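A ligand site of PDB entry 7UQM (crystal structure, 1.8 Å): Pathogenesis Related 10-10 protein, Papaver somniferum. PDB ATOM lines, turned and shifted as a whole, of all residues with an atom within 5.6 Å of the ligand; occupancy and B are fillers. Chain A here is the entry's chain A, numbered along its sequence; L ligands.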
ATOM      1  N   PRO A  37     -32.211 -19.124 -17.731  1.00  0.00           N
ATOM      2  CA  PRO A  37     -33.583 -19.647 -17.609  1.00  0.00           C
ATOM      3  C   PRO A  37     -34.436 -19.392 -18.850  1.00  0.00           C
ATOM      4  O   PRO A  37     -33.889 -19.398 -19.945  1.00  0.00           O
ATOM      5  CB  PRO A  37     -34.134 -18.900 -16.389  1.00  0.00           C
ATOM      6  CG  PRO A  37     -32.932 -18.448 -15.633  1.00  0.00           C
ATOM      7  CD  PRO A  37     -31.906 -18.128 -16.688  1.00  0.00           C
ATOM      8  N   ASN A  38     -35.740 -19.158 -18.704  1.00  0.00           N
ATOM      9  CA  ASN A  38     -36.695 -19.445 -19.776  1.00  0.00           C
ATOM     10  C   ASN A  38     -37.071 -18.189 -20.565  1.00  0.00           C
ATOM     11  O   ASN A  38     -38.222 -17.727 -20.558  1.00  0.00           O
ATOM     12  CB  ASN A  38     -37.927 -20.143 -19.213  1.00  0.00           C
ATOM     13  CG  ASN A  38     -38.363 -19.571 -17.877  1.00  0.00           C
ATOM     14  OD1 ASN A  38     -38.753 -20.317 -16.971  1.00  0.00           O
ATOM     15  ND2 ASN A  38     -38.287 -18.262 -17.727  1.00  0.00           N
ATOM     16  N   ILE A  40     -36.986 -18.820 -23.488  1.00  0.00           N
ATOM     17  CA  ILE A  40     -37.312 -19.753 -24.554  1.00  0.00           C
ATOM     18  C   ILE A  40     -38.192 -20.832 -23.933  1.00  0.00           C
ATOM     19  O   ILE A  40     -37.958 -21.238 -22.783  1.00  0.00           O
ATOM     20  CB  ILE A  40     -36.041 -20.326 -25.202  1.00  0.00           C
ATOM     21  CG1 ILE A  40     -35.569 -19.432 -26.363  1.00  0.00           C
ATOM     22  CG2 ILE A  40     -36.221 -21.772 -25.655  1.00  0.00           C
ATOM     23  CD1 ILE A  40     -36.602 -19.242 -27.444  1.00  0.00           C
ATOM     24  N   PRO A  41     -39.252 -21.289 -24.607  1.00  0.00           N
ATOM     25  CA  PRO A  41     -39.998 -22.437 -24.067  1.00  0.00           C
ATOM     26  C   PRO A  41     -39.087 -23.661 -24.076  1.00  0.00           C
ATOM     27  O   PRO A  41     -38.441 -23.952 -25.078  1.00  0.00           O
ATOM     28  CB  PRO A  41     -41.189 -22.601 -25.042  1.00  0.00           C
ATOM     29  CG  PRO A  41     -41.165 -21.355 -25.927  1.00  0.00           C
ATOM     30  CD  PRO A  41     -39.752 -20.855 -25.937  1.00  0.00           C
ATOM     31  N   HIS A  42     -38.996 -24.343 -22.935  1.00  0.00           N
ATOM     32  CA  HIS A  42     -38.062 -25.472 -22.920  1.00  0.00           C
ATOM     33  C   HIS A  42     -38.351 -26.325 -21.700  1.00  0.00           C
ATOM     34  O   HIS A  42     -38.868 -25.821 -20.688  1.00  0.00           O
ATOM     35  CB  HIS A  42     -36.588 -25.019 -22.946  1.00  0.00           C
ATOM     36  CG  HIS A  42     -36.148 -24.256 -21.727  1.00  0.00           C
ATOM     37  ND1 HIS A  42     -36.120 -24.826 -20.465  1.00  0.00           N
ATOM     38  CD2 HIS A  42     -35.720 -22.977 -21.577  1.00  0.00           C
ATOM     39  CE1 HIS A  42     -35.699 -23.925 -19.591  1.00  0.00           C
ATOM     40  NE2 HIS A  42     -35.437 -22.807 -20.247  1.00  0.00           N
ATOM     41  N   TRP A  63     -33.648 -32.568 -24.508  1.00  0.00           N
ATOM     42  CA  TRP A  63     -34.303 -31.285 -24.390  1.00  0.00           C
ATOM     43  C   TRP A  63     -35.472 -31.215 -25.348  1.00  0.00           C
ATOM     44  O   TRP A  63     -35.380 -31.727 -26.447  1.00  0.00           O
ATOM     45  CB  TRP A  63     -33.306 -30.180 -24.780  1.00  0.00           C
ATOM     46  CG  TRP A  63     -32.239 -29.938 -23.774  1.00  0.00           C
ATOM     47  CD1 TRP A  63     -31.041 -30.528 -23.719  1.00  0.00           C
ATOM     48  CD2 TRP A  63     -32.335 -29.064 -22.688  1.00  0.00           C
ATOM     49  NE1 TRP A  63     -30.337 -30.058 -22.625  1.00  0.00           N
ATOM     50  CE2 TRP A  63     -31.118 -29.144 -21.991  1.00  0.00           C
ATOM     51  CE3 TRP A  63     -33.309 -28.148 -22.268  1.00  0.00           C
ATOM     52  CZ2 TRP A  63     -30.844 -28.334 -20.885  1.00  0.00           C
ATOM     53  CZ3 TRP A  63     -33.038 -27.354 -21.133  1.00  0.00           C
ATOM     54  CH2 TRP A  63     -31.828 -27.483 -20.446  1.00  0.00           C
ATOM     55  N   TYR A  65     -37.573 -27.924 -26.906  1.00  0.00           N
ATOM     56  CA  TYR A  65     -37.400 -26.483 -26.825  1.00  0.00           C
ATOM     57  C   TYR A  65     -37.921 -25.876 -28.116  1.00  0.00           C
ATOM     58  O   TYR A  65     -38.121 -26.578 -29.119  1.00  0.00           O
ATOM     59  CB  TYR A  65     -35.915 -26.086 -26.614  1.00  0.00           C
ATOM     60  CG  TYR A  65     -35.014 -26.473 -27.749  1.00  0.00           C
ATOM     61  CD1 TYR A  65     -34.619 -25.542 -28.735  1.00  0.00           C
ATOM     62  CD2 TYR A  65     -34.513 -27.752 -27.825  1.00  0.00           C
ATOM     63  CE1 TYR A  65     -33.778 -25.958 -29.809  1.00  0.00           C
ATOM     64  CE2 TYR A  65     -33.691 -28.141 -28.831  1.00  0.00           C
ATOM     65  CZ  TYR A  65     -33.318 -27.249 -29.810  1.00  0.00           C
ATOM     66  OH  TYR A  65     -32.516 -27.702 -30.771  1.00  0.00           O
ATOM     67  N   ALA A  74     -33.329 -32.265 -28.723  1.00  0.00           N
ATOM     68  CA  ALA A  74     -31.909 -32.587 -28.850  1.00  0.00           C
ATOM     69  C   ALA A  74     -31.515 -33.445 -27.660  1.00  0.00           C
ATOM     70  O   ALA A  74     -32.010 -33.190 -26.559  1.00  0.00           O
ATOM     71  CB  ALA A  74     -31.026 -31.338 -28.866  1.00  0.00           C
ATOM     72  N   GLU A  76     -28.274 -34.220 -25.383  1.00  0.00           N
ATOM     73  CA  GLU A  76     -27.049 -33.494 -25.068  1.00  0.00           C
ATOM     74  C   GLU A  76     -26.358 -34.229 -23.935  1.00  0.00           C
ATOM     75  O   GLU A  76     -27.001 -34.502 -22.922  1.00  0.00           O
ATOM     76  CB  GLU A  76     -27.358 -32.065 -24.590  1.00  0.00           C
ATOM     77  CG  GLU A  76     -26.253 -31.340 -23.762  1.00  0.00           C
ATOM     78  CD  GLU A  76     -26.772 -30.091 -23.144  1.00  0.00           C
ATOM     79  OE1 GLU A  76     -26.407 -28.962 -23.627  1.00  0.00           O
ATOM     80  OE2 GLU A  76     -27.534 -30.210 -22.157  1.00  0.00           O
ATOM     81  N   HIS A  89     -20.780 -29.395 -24.085  1.00  0.00           N
ATOM     82  CA  HIS A  89     -22.097 -29.956 -24.349  1.00  0.00           C
ATOM     83  C   HIS A  89     -22.024 -30.646 -25.712  1.00  0.00           C
ATOM     84  O   HIS A  89     -21.810 -29.973 -26.743  1.00  0.00           O
ATOM     85  CB  HIS A  89     -23.211 -28.890 -24.415  1.00  0.00           C
ATOM     86  CG  HIS A  89     -23.238 -27.925 -23.281  1.00  0.00           C
ATOM     87  ND1 HIS A  89     -23.828 -28.251 -22.084  1.00  0.00           N
ATOM     88  CD2 HIS A  89     -22.949 -26.607 -23.204  1.00  0.00           C
ATOM     89  CE1 HIS A  89     -23.827 -27.208 -21.286  1.00  0.00           C
ATOM     90  NE2 HIS A  89     -23.308 -26.189 -21.932  1.00  0.00           N
ATOM     91  N   HIS A  90     -22.203 -31.953 -25.727  1.00  0.00           N
ATOM     92  CA  HIS A  90     -22.017 -32.778 -26.914  1.00  0.00           C
ATOM     93  C   HIS A  90     -23.387 -33.242 -27.393  1.00  0.00           C
ATOM     94  O   HIS A  90     -24.051 -33.971 -26.684  1.00  0.00           O
ATOM     95  CB  HIS A  90     -21.148 -33.993 -26.563  1.00  0.00           C
ATOM     96  CG  HIS A  90     -20.999 -34.989 -27.690  1.00  0.00           C
ATOM     97  ND1 HIS A  90     -20.404 -34.700 -28.893  1.00  0.00           N
ATOM     98  CD2 HIS A  90     -21.310 -36.312 -27.738  1.00  0.00           C
ATOM     99  CE1 HIS A  90     -20.391 -35.783 -29.664  1.00  0.00           C
ATOM    100  NE2 HIS A  90     -20.932 -36.780 -28.973  1.00  0.00           N
ATOM    101  N   ILE A  91     -23.829 -32.801 -28.580  1.00  0.00           N
ATOM    102  CA  ILE A  91     -25.151 -33.151 -29.063  1.00  0.00           C
ATOM    103  C   ILE A  91     -25.058 -34.455 -29.889  1.00  0.00           C
ATOM    104  O   ILE A  91     -24.214 -34.590 -30.773  1.00  0.00           O
ATOM    105  CB  ILE A  91     -25.755 -32.005 -29.921  1.00  0.00           C
ATOM    106  CG1 ILE A  91     -25.938 -30.734 -29.105  1.00  0.00           C
ATOM    107  CG2 ILE A  91     -27.129 -32.490 -30.491  1.00  0.00           C
ATOM    108  CD1 ILE A  91     -26.822 -30.927 -27.885  1.00  0.00           C
ATOM    109  N   ALA A  96     -31.029 -30.513 -34.789  1.00  0.00           N
ATOM    110  CA  ALA A  96     -29.779 -29.989 -35.294  1.00  0.00           C
ATOM    111  C   ALA A  96     -29.012 -31.039 -36.091  1.00  0.00           C
ATOM    112  O   ALA A  96     -28.217 -30.682 -36.966  1.00  0.00           O
ATOM    113  CB  ALA A  96     -28.918 -29.486 -34.165  1.00  0.00           C
ATOM    114  N   PHE A 103     -21.919 -31.519 -33.670  1.00  0.00           N
ATOM    115  CA  PHE A 103     -22.359 -30.239 -33.098  1.00  0.00           C
ATOM    116  C   PHE A 103     -21.978 -30.285 -31.628  1.00  0.00           C
ATOM    117  O   PHE A 103     -22.553 -31.078 -30.873  1.00  0.00           O
ATOM    118  CB  PHE A 103     -23.881 -30.070 -33.258  1.00  0.00           C
ATOM    119  CG  PHE A 103     -24.402 -28.705 -32.835  1.00  0.00           C
ATOM    120  CD1 PHE A 103     -24.602 -27.722 -33.796  1.00  0.00           C
ATOM    121  CD2 PHE A 103     -24.749 -28.406 -31.545  1.00  0.00           C
ATOM    122  CE1 PHE A 103     -25.128 -26.500 -33.473  1.00  0.00           C
ATOM    123  CE2 PHE A 103     -25.270 -27.156 -31.220  1.00  0.00           C
ATOM    124  CZ  PHE A 103     -25.479 -26.196 -32.229  1.00  0.00           C
ATOM    125  N   ASP A 104     -21.034 -29.461 -31.227  1.00  0.00           N
ATOM    126  CA  ASP A 104     -20.577 -29.386 -29.834  1.00  0.00           C
ATOM    127  C   ASP A 104     -20.513 -27.945 -29.394  1.00  0.00           C
ATOM    128  O   ASP A 104     -20.195 -27.076 -30.235  1.00  0.00           O
ATOM    129  CB  ASP A 104     -19.215 -29.973 -29.660  1.00  0.00           C
ATOM    130  CG  ASP A 104     -19.200 -31.473 -29.907  1.00  0.00           C
ATOM    131  OD1 ASP A 104     -19.632 -32.206 -29.061  1.00  0.00           O
ATOM    132  OD2 ASP A 104     -18.737 -31.935 -30.953  1.00  0.00           O
ATOM    133  N   VAL A 105     -20.819 -27.681 -28.119  1.00  0.00           N
ATOM    134  CA  VAL A 105     -20.788 -26.306 -27.593  1.00  0.00           C
ATOM    135  C   VAL A 105     -19.889 -26.300 -26.386  1.00  0.00           C
ATOM    136  O   VAL A 105     -20.126 -27.049 -25.425  1.00  0.00           O
ATOM    137  CB  VAL A 105     -22.203 -25.792 -27.245  1.00  0.00           C
ATOM    138  CG1 VAL A 105     -22.190 -24.348 -26.718  1.00  0.00           C
ATOM    139  CG2 VAL A 105     -23.147 -25.898 -28.447  1.00  0.00           C
ATOM    140  N   TYR A 139     -28.294 -20.768 -33.271  1.00  0.00           N
ATOM    141  CA  TYR A 139     -27.826 -21.223 -31.953  1.00  0.00           C
ATOM    142  C   TYR A 139     -26.851 -20.243 -31.306  1.00  0.00           C
ATOM    143  O   TYR A 139     -26.942 -20.021 -30.111  1.00  0.00           O
ATOM    144  CB  TYR A 139     -27.198 -22.612 -32.029  1.00  0.00           C
ATOM    145  CG  TYR A 139     -28.275 -23.683 -32.270  1.00  0.00           C
ATOM    146  CD1 TYR A 139     -29.096 -24.113 -31.217  1.00  0.00           C
ATOM    147  CD2 TYR A 139     -28.532 -24.151 -33.548  1.00  0.00           C
ATOM    148  CE1 TYR A 139     -30.097 -25.039 -31.460  1.00  0.00           C
ATOM    149  CE2 TYR A 139     -29.532 -25.092 -33.775  1.00  0.00           C
ATOM    150  CZ  TYR A 139     -30.273 -25.545 -32.716  1.00  0.00           C
ATOM    151  OH  TYR A 139     -31.286 -26.453 -32.978  1.00  0.00           O
ATOM    152  N   PHE A 142     -28.827 -17.562 -29.792  1.00  0.00           N
ATOM    153  CA  PHE A 142     -29.564 -18.067 -28.626  1.00  0.00           C
ATOM    154  C   PHE A 142     -28.651 -18.159 -27.393  1.00  0.00           C
ATOM    155  O   PHE A 142     -29.014 -17.675 -26.310  1.00  0.00           O
ATOM    156  CB  PHE A 142     -30.183 -19.433 -28.959  1.00  0.00           C
ATOM    157  CG  PHE A 142     -30.731 -20.137 -27.741  1.00  0.00           C
ATOM    158  CD1 PHE A 142     -31.939 -19.757 -27.176  1.00  0.00           C
ATOM    159  CD2 PHE A 142     -30.003 -21.121 -27.131  1.00  0.00           C
ATOM    160  CE1 PHE A 142     -32.405 -20.385 -26.019  1.00  0.00           C
ATOM    161  CE2 PHE A 142     -30.467 -21.771 -25.965  1.00  0.00           C
ATOM    162  CZ  PHE A 142     -31.656 -21.394 -25.423  1.00  0.00           C
ATOM    163  N   PHE A 143     -27.500 -18.798 -27.536  1.00  0.00           N
ATOM    164  CA  PHE A 143     -26.588 -18.969 -26.409  1.00  0.00           C
ATOM    165  C   PHE A 143     -26.065 -17.616 -25.938  1.00  0.00           C
ATOM    166  O   PHE A 143     -25.914 -17.382 -24.745  1.00  0.00           O
ATOM    167  CB  PHE A 143     -25.432 -19.900 -26.801  1.00  0.00           C
ATOM    168  CG  PHE A 143     -25.864 -21.314 -26.961  1.00  0.00           C
ATOM    169  CD1 PHE A 143     -26.597 -21.880 -25.960  1.00  0.00           C
ATOM    170  CD2 PHE A 143     -25.595 -22.029 -28.102  1.00  0.00           C
ATOM    171  CE1 PHE A 143     -27.051 -23.171 -26.075  1.00  0.00           C
ATOM    172  CE2 PHE A 143     -26.077 -23.353 -28.190  1.00  0.00           C
ATOM    173  CZ  PHE A 143     -26.788 -23.879 -27.195  1.00  0.00           C
ATOM    174  N   ASN A 146     -28.634 -15.877 -23.946  1.00  0.00           N
ATOM    175  CA  ASN A 146     -28.785 -16.558 -22.675  1.00  0.00           C
ATOM    176  C   ASN A 146     -27.700 -16.152 -21.683  1.00  0.00           C
ATOM    177  O   ASN A 146     -28.006 -15.836 -20.528  1.00  0.00           O
ATOM    178  CB  ASN A 146     -28.814 -18.064 -22.922  1.00  0.00           C
ATOM    179  CG  ASN A 146     -29.075 -18.868 -21.661  1.00  0.00           C
ATOM    180  OD1 ASN A 146     -30.193 -19.263 -21.386  1.00  0.00           O
ATOM    181  ND2 ASN A 146     -28.018 -19.111 -20.888  1.00  0.00           N
HETATM  182  C1  LIG L   1     -25.314 -27.882 -26.878  1.00  0.00           C
HETATM  183  O1  LIG L   1     -26.234 -27.511 -27.864  1.00  0.00           O
HETATM  184  C2  LIG L   1     -27.555 -27.496 -27.441  1.00  0.00           C
HETATM  185  C3  LIG L   1     -28.554 -27.516 -28.413  1.00  0.00           C
HETATM  186  O2  LIG L   1     -28.137 -27.561 -29.714  1.00  0.00           O
HETATM  187  C4  LIG L   1     -28.933 -28.242 -30.648  1.00  0.00           C
HETATM  188  C5  LIG L   1     -29.869 -27.495 -28.093  1.00  0.00           C
HETATM  189  C6  LIG L   1     -30.243 -27.398 -26.821  1.00  0.00           C
HETATM  190  C7  LIG L   1     -27.873 -27.432 -26.074  1.00  0.00           C
HETATM  191  C8  LIG L   1     -29.265 -27.397 -25.834  1.00  0.00           C
HETATM  192  C9  LIG L   1     -29.797 -27.388 -24.448  1.00  0.00           C
HETATM  193  C10 LIG L   1     -29.078 -26.469 -23.517  1.00  0.00           C
HETATM  194  N1  LIG L   1     -27.865 -26.766 -23.087  1.00  0.00           N
HETATM  195  C11 LIG L   1     -27.323 -25.847 -22.267  1.00  0.00           C
HETATM  196  C12 LIG L   1     -27.964 -24.689 -21.874  1.00  0.00           C
HETATM  197  C13 LIG L   1     -29.238 -24.435 -22.342  1.00  0.00           C
HETATM  198  C14 LIG L   1     -29.818 -25.366 -23.184  1.00  0.00           C
HETATM  199  C15 LIG L   1     -31.096 -25.228 -23.737  1.00  0.00           C
HETATM  200  C16 LIG L   1     -31.783 -24.087 -23.376  1.00  0.00           C
HETATM  201  O3  LIG L   1     -33.059 -23.872 -23.890  1.00  0.00           O
HETATM  202  C17 LIG L   1     -33.257 -24.522 -25.111  1.00  0.00           C
HETATM  203  C18 LIG L   1     -31.267 -23.123 -22.519  1.00  0.00           C
HETATM  204  C19 LIG L   1     -29.979 -23.289 -22.008  1.00  0.00           C
HETATM  205  O4  LIG L   1     -32.041 -21.999 -22.198  1.00  0.00           O
HETATM  206  C20 LIG L   1     -32.301 -21.860 -20.824  1.00  0.00           C
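The side-chain carboxylate of Glu 76 is in hydrogen-bond range of a nitrogen (N1) of the ligand (2.7 Å). The side-chain amide oxygen of Asn 146 sits close to an oxygen (O4) of the ligand (3.4 Å).
The backbone carbonyl oxygen of Val 105 lies within hydrogen-bond range of the backbone NH of His 89, 2.8 Å away. OE2 of Glu 76 sits at hydrogen-bond distance from NE1 of Trp 63 (2.8 Å). N of Ile 91 sits at hydrogen-bond distance from O of Phe 103, at 3.1 Å. N of Trp 63 lies within hydrogen-bond range of O of Ala 74, 2.7 Å away. The side-chain hydroxyl (OH) of Tyr 65 is in hydrogen-bond range of the side-chain hydroxyl (OH) of Tyr 139 (2.8 Å). The side-chain carboxylate of Glu 76 sits at hydrogen-bond distance from a ring nitrogen (ND1) of His 89, 3.1 Å away.
O of Pro 37 touches C20 of the ligand (3.1 Å). His 42 touches the ligand. NE1 of Trp 63 touches C9 of the ligand, 3.3 Å away. Tyr 65 touches the ligand. CB of His 89 touches C1 of the ligand, 3.4 Å away. Ile 91 touches the ligand. Ala 96 touches the ligand. Phe 103 touches the ligand. CG2 of Val 105 touches C1 of the ligand, 3.3 Å away. CE1 of Tyr 139 touches C4 of the ligand, 3.5 Å away. CZ of Phe 142 touches O3 of the ligand (3.2 Å). Phe 143 touches the ligand. Within 4 Å of the ligand: Pro 37, His 42, Trp 63, Tyr 65, Glu 76, His 89, Ile 91, Ala 96, Phe 103, Val 105, Tyr 139, Phe 142, Phe 143 and Asn 146.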
